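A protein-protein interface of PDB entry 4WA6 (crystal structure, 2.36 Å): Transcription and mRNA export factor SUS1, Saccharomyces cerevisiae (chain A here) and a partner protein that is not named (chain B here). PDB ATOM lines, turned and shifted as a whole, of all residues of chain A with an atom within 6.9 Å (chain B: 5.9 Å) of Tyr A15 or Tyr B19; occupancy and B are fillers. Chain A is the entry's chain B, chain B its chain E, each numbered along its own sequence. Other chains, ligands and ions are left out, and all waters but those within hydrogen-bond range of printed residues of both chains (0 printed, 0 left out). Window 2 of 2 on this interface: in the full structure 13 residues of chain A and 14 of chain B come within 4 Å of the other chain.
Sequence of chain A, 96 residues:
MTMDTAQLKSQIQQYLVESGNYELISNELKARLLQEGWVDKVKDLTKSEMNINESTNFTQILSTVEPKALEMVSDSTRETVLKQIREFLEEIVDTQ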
ATOM      1  N   SER A  10      14.493   6.991   1.058  1.00  0.00           N
ATOM      2  CA  SER A  10      14.097   8.050   0.162  1.00  0.00           C
ATOM      3  C   SER A  10      12.614   8.415   0.168  1.00  0.00           C
ATOM      4  O   SER A  10      12.282   9.587   0.091  1.00  0.00           O
ATOM      5  CB  SER A  10      14.473   7.632  -1.251  1.00  0.00           C
ATOM      6  OG  SER A  10      14.762   8.794  -1.971  1.00  0.00           O
ATOM      7  N   GLN A  11      11.708   7.435   0.252  1.00  0.00           N
ATOM      8  CA  GLN A  11      10.284   7.762   0.358  1.00  0.00           C
ATOM      9  C   GLN A  11      10.023   8.488   1.665  1.00  0.00           C
ATOM     10  O   GLN A  11       9.276   9.486   1.692  1.00  0.00           O
ATOM     11  CB  GLN A  11       9.380   6.515   0.290  1.00  0.00           C
ATOM     12  CG  GLN A  11       9.208   5.925  -1.107  1.00  0.00           C
ATOM     13  CD  GLN A  11       9.077   4.407  -1.129  1.00  0.00           C
ATOM     14  OE1 GLN A  11       8.706   3.777  -0.133  1.00  0.00           O
ATOM     15  NE2 GLN A  11       9.383   3.808  -2.288  1.00  0.00           N
ATOM     16  N   ILE A  12      10.645   8.018   2.742  1.00  0.00           N
ATOM     17  CA  ILE A  12      10.362   8.605   4.028  1.00  0.00           C
ATOM     18  C   ILE A  12      10.698  10.116   4.007  1.00  0.00           C
ATOM     19  O   ILE A  12       9.861  10.983   4.335  1.00  0.00           O
ATOM     20  CB  ILE A  12      11.076   7.827   5.142  1.00  0.00           C
ATOM     21  CG1 ILE A  12      10.476   6.429   5.296  1.00  0.00           C
ATOM     22  CG2 ILE A  12      10.933   8.526   6.468  1.00  0.00           C
ATOM     23  CD1 ILE A  12      11.183   5.571   6.333  1.00  0.00           C
ATOM     24  N   GLN A  13      11.905  10.426   3.532  1.00  0.00           N
ATOM     25  CA  GLN A  13      12.367  11.814   3.436  1.00  0.00           C
ATOM     26  C   GLN A  13      11.396  12.611   2.568  1.00  0.00           C
ATOM     27  O   GLN A  13      10.958  13.715   2.897  1.00  0.00           O
ATOM     28  CB  GLN A  13      13.786  11.847   2.869  1.00  0.00           C
ATOM     29  CG  GLN A  13      14.824  11.369   3.870  1.00  0.00           C
ATOM     30  CD  GLN A  13      16.240  11.296   3.308  1.00  0.00           C
ATOM     31  OE1 GLN A  13      16.485  11.723   2.212  1.00  0.00           O
ATOM     32  NE2 GLN A  13      17.159  10.691   4.058  1.00  0.00           N
ATOM     33  N   GLN A  14      11.014  12.014   1.464  1.00  0.00           N
ATOM     34  CA  GLN A  14      10.040  12.634   0.591  1.00  0.00           C
ATOM     35  C   GLN A  14       8.694  12.861   1.229  1.00  0.00           C
ATOM     36  O   GLN A  14       8.107  13.906   1.037  1.00  0.00           O
ATOM     37  CB  GLN A  14       9.937  11.791  -0.669  1.00  0.00           C
ATOM     38  CG  GLN A  14       8.924  12.209  -1.687  1.00  0.00           C
ATOM     39  CD  GLN A  14       9.308  11.672  -3.057  1.00  0.00           C
ATOM     40  OE1 GLN A  14      10.513  11.485  -3.370  1.00  0.00           O
ATOM     41  NE2 GLN A  14       8.310  11.428  -3.883  1.00  0.00           N
ATOM     42  N   TYR A  15       8.163  11.913   1.989  1.00  0.00           N
ATOM     43  CA  TYR A  15       6.876  12.203   2.643  1.00  0.00           C
ATOM     44  C   TYR A  15       7.014  13.355   3.658  1.00  0.00           C
ATOM     45  O   TYR A  15       6.148  14.261   3.741  1.00  0.00           O
ATOM     46  CB  TYR A  15       6.278  10.978   3.297  1.00  0.00           C
ATOM     47  CG  TYR A  15       5.561  10.097   2.320  1.00  0.00           C
ATOM     48  CD1 TYR A  15       4.236  10.333   1.975  1.00  0.00           C
ATOM     49  CD2 TYR A  15       6.188   8.993   1.770  1.00  0.00           C
ATOM     50  CE1 TYR A  15       3.576   9.501   1.078  1.00  0.00           C
ATOM     51  CE2 TYR A  15       5.551   8.174   0.859  1.00  0.00           C
ATOM     52  CZ  TYR A  15       4.258   8.420   0.519  1.00  0.00           C
ATOM     53  OH  TYR A  15       3.666   7.563  -0.377  1.00  0.00           O
ATOM     54  N   LEU A  16       8.128  13.346   4.381  1.00  0.00           N
ATOM     55  CA  LEU A  16       8.459  14.439   5.295  1.00  0.00           C
ATOM     56  C   LEU A  16       8.373  15.759   4.601  1.00  0.00           C
ATOM     57  O   LEU A  16       7.787  16.699   5.132  1.00  0.00           O
ATOM     58  CB  LEU A  16       9.850  14.267   5.861  1.00  0.00           C
ATOM     59  CG  LEU A  16       9.991  13.467   7.153  1.00  0.00           C
ATOM     60  CD1 LEU A  16      11.468  13.436   7.567  1.00  0.00           C
ATOM     61  CD2 LEU A  16       9.148  14.066   8.266  1.00  0.00           C
ATOM     62  N   VAL A  17       8.920  15.818   3.392  1.00  0.00           N
ATOM     63  CA  VAL A  17       8.929  17.045   2.617  1.00  0.00           C
ATOM     64  C   VAL A  17       7.530  17.465   2.163  1.00  0.00           C
ATOM     65  O   VAL A  17       7.147  18.625   2.294  1.00  0.00           O
ATOM     66  CB  VAL A  17       9.908  16.960   1.412  1.00  0.00           C
ATOM     67  CG1 VAL A  17       9.878  18.251   0.619  1.00  0.00           C
ATOM     68  CG2 VAL A  17      11.344  16.737   1.890  1.00  0.00           C
ATOM     69  N   GLU A  18       6.755  16.518   1.662  1.00  0.00           N
ATOM     70  CA  GLU A  18       5.388  16.804   1.175  1.00  0.00           C
ATOM     71  C   GLU A  18       4.391  17.218   2.257  1.00  0.00           C
ATOM     72  O   GLU A  18       3.493  17.997   1.961  1.00  0.00           O
ATOM     73  CB  GLU A  18       4.833  15.627   0.375  1.00  0.00           C
ATOM     74  CG  GLU A  18       5.768  15.171  -0.732  1.00  0.00           C
ATOM     75  CD  GLU A  18       5.268  15.474  -2.116  1.00  0.00           C
ATOM     76  OE1 GLU A  18       4.455  16.415  -2.308  1.00  0.00           O
ATOM     77  OE2 GLU A  18       5.677  14.739  -3.030  1.00  0.00           O
ATOM     78  N   SER A  19       4.527  16.707   3.485  1.00  0.00           N
ATOM     79  CA  SER A  19       3.713  17.202   4.618  1.00  0.00           C
ATOM     80  C   SER A  19       3.997  18.694   4.961  1.00  0.00           C
ATOM     81  O   SER A  19       3.133  19.403   5.363  1.00  0.00           O
ATOM     82  CB  SER A  19       3.896  16.317   5.863  1.00  0.00           C
ATOM     83  OG  SER A  19       5.254  16.253   6.316  1.00  0.00           O
ATOM     84  N   GLY A  20       5.219  19.161   4.763  1.00  0.00           N
ATOM     85  CA  GLY A  20       5.634  20.475   5.238  1.00  0.00           C
ATOM     86  C   GLY A  20       6.521  20.284   6.462  1.00  0.00           C
ATOM     87  O   GLY A  20       7.179  21.228   6.908  1.00  0.00           O
ATOM     88  N   ASN A  21       6.562  19.068   6.996  1.00  0.00           N
ATOM     89  CA  ASN A  21       7.271  18.831   8.252  1.00  0.00           C
ATOM     90  C   ASN A  21       8.768  18.854   8.148  1.00  0.00           C
ATOM     91  O   ASN A  21       9.442  19.119   9.144  1.00  0.00           O
ATOM     92  CB  ASN A  21       6.808  17.528   8.914  1.00  0.00           C
ATOM     93  CG  ASN A  21       5.323  17.571   9.292  1.00  0.00           C
ATOM     94  OD1 ASN A  21       4.790  18.651   9.566  1.00  0.00           O
ATOM     95  ND2 ASN A  21       4.663  16.412   9.316  1.00  0.00           N
ATOM     96  N   TYR A  22       9.305  18.619   6.952  1.00  0.00           N
ATOM     97  CA  TYR A  22      10.778  18.753   6.727  1.00  0.00           C
ATOM     98  C   TYR A  22      11.179  20.192   6.879  1.00  0.00           C
ATOM     99  O   TYR A  22      12.189  20.499   7.488  1.00  0.00           O
ATOM    100  CB  TYR A  22      11.167  18.245   5.332  1.00  0.00           C
ATOM    101  CG  TYR A  22      12.640  17.989   5.157  1.00  0.00           C
ATOM    102  CD1 TYR A  22      13.199  16.775   5.536  1.00  0.00           C
ATOM    103  CD2 TYR A  22      13.463  18.929   4.583  1.00  0.00           C
ATOM    104  CE1 TYR A  22      14.572  16.508   5.381  1.00  0.00           C
ATOM    105  CE2 TYR A  22      14.825  18.697   4.443  1.00  0.00           C
ATOM    106  CZ  TYR A  22      15.379  17.479   4.826  1.00  0.00           C
ATOM    107  OH  TYR A  22      16.703  17.195   4.634  1.00  0.00           O
ATOM    108  N   ILE A  92       4.301   8.402   9.772  1.00  0.00           N
ATOM    109  CA  ILE A  92       4.520   8.017   8.392  1.00  0.00           C
ATOM    110  C   ILE A  92       4.716   6.498   8.215  1.00  0.00           C
ATOM    111  O   ILE A  92       4.287   5.945   7.209  1.00  0.00           O
ATOM    112  CB  ILE A  92       5.766   8.775   7.859  1.00  0.00           C
ATOM    113  CG1 ILE A  92       5.462  10.270   7.682  1.00  0.00           C
ATOM    114  CG2 ILE A  92       6.269   8.219   6.528  1.00  0.00           C
ATOM    115  CD1 ILE A  92       6.708  11.118   7.566  1.00  0.00           C
ATOM    116  N   ILE B  11       6.035   2.167   4.574  1.00  0.00           N
ATOM    117  CA  ILE B  11       5.229   3.369   4.781  1.00  0.00           C
ATOM    118  C   ILE B  11       3.785   2.996   5.031  1.00  0.00           C
ATOM    119  O   ILE B  11       3.276   2.098   4.417  1.00  0.00           O
ATOM    120  CB  ILE B  11       5.368   4.304   3.566  1.00  0.00           C
ATOM    121  CG1 ILE B  11       6.692   5.015   3.705  1.00  0.00           C
ATOM    122  CG2 ILE B  11       4.290   5.356   3.555  1.00  0.00           C
ATOM    123  CD1 ILE B  11       7.188   5.621   2.437  1.00  0.00           C
ATOM    124  N   VAL B  15      -1.175   6.429   4.954  1.00  0.00           N
ATOM    125  CA  VAL B  15      -0.516   7.652   4.481  1.00  0.00           C
ATOM    126  C   VAL B  15      -0.333   7.677   2.958  1.00  0.00           C
ATOM    127  O   VAL B  15      -0.319   8.750   2.349  1.00  0.00           O
ATOM    128  CB  VAL B  15       0.899   7.850   5.129  1.00  0.00           C
ATOM    129  CG1 VAL B  15       1.603   9.078   4.562  1.00  0.00           C
ATOM    130  CG2 VAL B  15       0.816   7.972   6.648  1.00  0.00           C
ATOM    131  N   ILE B  16      -0.146   6.513   2.354  1.00  0.00           N
ATOM    132  CA  ILE B  16       0.036   6.443   0.913  1.00  0.00           C
ATOM    133  C   ILE B  16      -1.271   6.890   0.255  1.00  0.00           C
ATOM    134  O   ILE B  16      -1.285   7.723  -0.639  1.00  0.00           O
ATOM    135  CB  ILE B  16       0.406   5.018   0.454  1.00  0.00           C
ATOM    136  CG1 ILE B  16       1.741   4.585   1.092  1.00  0.00           C
ATOM    137  CG2 ILE B  16       0.476   4.972  -1.059  1.00  0.00           C
ATOM    138  CD1 ILE B  16       2.287   3.247   0.635  1.00  0.00           C
ATOM    139  N   GLU B  17      -2.360   6.328   0.743  1.00  0.00           N
ATOM    140  CA  GLU B  17      -3.726   6.690   0.364  1.00  0.00           C
ATOM    141  C   GLU B  17      -4.048   8.195   0.417  1.00  0.00           C
ATOM    142  O   GLU B  17      -5.090   8.611  -0.069  1.00  0.00           O
ATOM    143  CB  GLU B  17      -4.670   5.967   1.331  1.00  0.00           C
ATOM    144  CG  GLU B  17      -6.110   5.806   0.899  1.00  0.00           C
ATOM    145  CD  GLU B  17      -6.956   5.190   2.003  1.00  0.00           C
ATOM    146  OE1 GLU B  17      -8.115   5.627   2.190  1.00  0.00           O
ATOM    147  OE2 GLU B  17      -6.453   4.285   2.705  1.00  0.00           O
ATOM    148  N   GLU B  18      -3.188   8.990   1.054  1.00  0.00           N
ATOM    149  CA  GLU B  18      -3.374  10.439   1.187  1.00  0.00           C
ATOM    150  C   GLU B  18      -2.283  11.262   0.464  1.00  0.00           C
ATOM    151  O   GLU B  18      -2.373  12.474   0.442  1.00  0.00           O
ATOM    152  CB  GLU B  18      -3.532  10.802   2.691  1.00  0.00           C
ATOM    153  CG  GLU B  18      -2.527  11.790   3.303  1.00  0.00           C
ATOM    154  CD  GLU B  18      -2.698  11.988   4.818  1.00  0.00           C
ATOM    155  OE1 GLU B  18      -2.895  10.995   5.563  1.00  0.00           O
ATOM    156  OE2 GLU B  18      -2.623  13.151   5.280  1.00  0.00           O
ATOM    157  N   TYR B  19      -1.266  10.624  -0.131  1.00  0.00           N
ATOM    158  CA  TYR B  19      -0.307  11.328  -1.015  1.00  0.00           C
ATOM    159  C   TYR B  19       0.130  10.460  -2.177  1.00  0.00           C
ATOM    160  O   TYR B  19       0.795   9.445  -1.974  1.00  0.00           O
ATOM    161  CB  TYR B  19       0.990  11.776  -0.305  1.00  0.00           C
ATOM    162  CG  TYR B  19       0.849  12.848   0.754  1.00  0.00           C
ATOM    163  CD1 TYR B  19       0.183  14.052   0.487  1.00  0.00           C
ATOM    164  CD2 TYR B  19       1.412  12.669   2.034  1.00  0.00           C
ATOM    165  CE1 TYR B  19       0.056  15.029   1.475  1.00  0.00           C
ATOM    166  CE2 TYR B  19       1.291  13.636   3.021  1.00  0.00           C
ATOM    167  CZ  TYR B  19       0.615  14.807   2.736  1.00  0.00           C
ATOM    168  OH  TYR B  19       0.491  15.747   3.706  1.00  0.00           O
ATOM    169  N   SER B  20      -0.280  10.866  -3.380  1.00  0.00           N
ATOM    170  CA  SER B  20       0.424  10.583  -4.640  1.00  0.00           C
ATOM    171  C   SER B  20       0.568   9.107  -5.023  1.00  0.00           C
ATOM    172  O   SER B  20       0.597   8.219  -4.172  1.00  0.00           O
ATOM    173  CB  SER B  20       1.789  11.253  -4.604  1.00  0.00           C
ATOM    174  OG  SER B  20       2.471  10.873  -3.437  1.00  0.00           O
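Tyr A15 touches just these residues of chain B: Ile B11 (3.4 Å), Val B15 (3.9 Å), Ile B16 (3.8 Å) and Tyr B19 (3.7 Å).
Of the printed residues of chain A, Tyr B19 touches Tyr A15 (3.7 Å) and Ser A19 (3.7 Å).
Of the printed residues of chain B, Ile A92 touches Ile B11 (3.7 Å).
Printed residues of chain B within 4 Å of Ser A19: Tyr B19.
The nearest residue of chain B that does not touch Tyr A15 is Ser B20 (4.7 Å).
The side-chain hydroxyl of Ser A19 is in hydrogen-bond range of the backbone carbonyl oxygen of Leu A16 (2.8 Å).
The side-chain amide nitrogen (ND2) of Asn A21 is in hydrogen-bond range of the side-chain hydroxyl (OG) of Ser A19 (3.1 Å).
O of Tyr A15 is in hydrogen-bond range of OG of Ser A19 (3.4 Å).
Gln A11 touches Ile B11.
Ile B11 touches Tyr A15.
Val B15 touches Tyr A15.
OH of Tyr A15 touches CG1 of Ile B16, 3.8 Å away.
Tyr B19 touches Tyr A15 (CD2 to CD1, 3.7 Å).
Tyr B19 touches Ser A19.
Ile A92 touches Ile B11 (O to CA, 3.7 Å).
Of the 14 printed residues of chain A, 4 touch a printed residue of chain B.
Printed residues of chain A that touch a printed residue of chain B: Gln A11, Tyr A15, Ser A19 and Ile A92.
Along chain A the printed residues that touch a printed residue of chain B span positions 11 to 92.
Printed residues of chain B that touch a printed residue of chain A: Ile B11, Val B15, Ile B16 and Tyr B19.
Hydrophobic or aromatic side chains of chain B within 4 Å of the printed part of chain A: Ile B11, Val B15, Ile B16 and Tyr B19.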
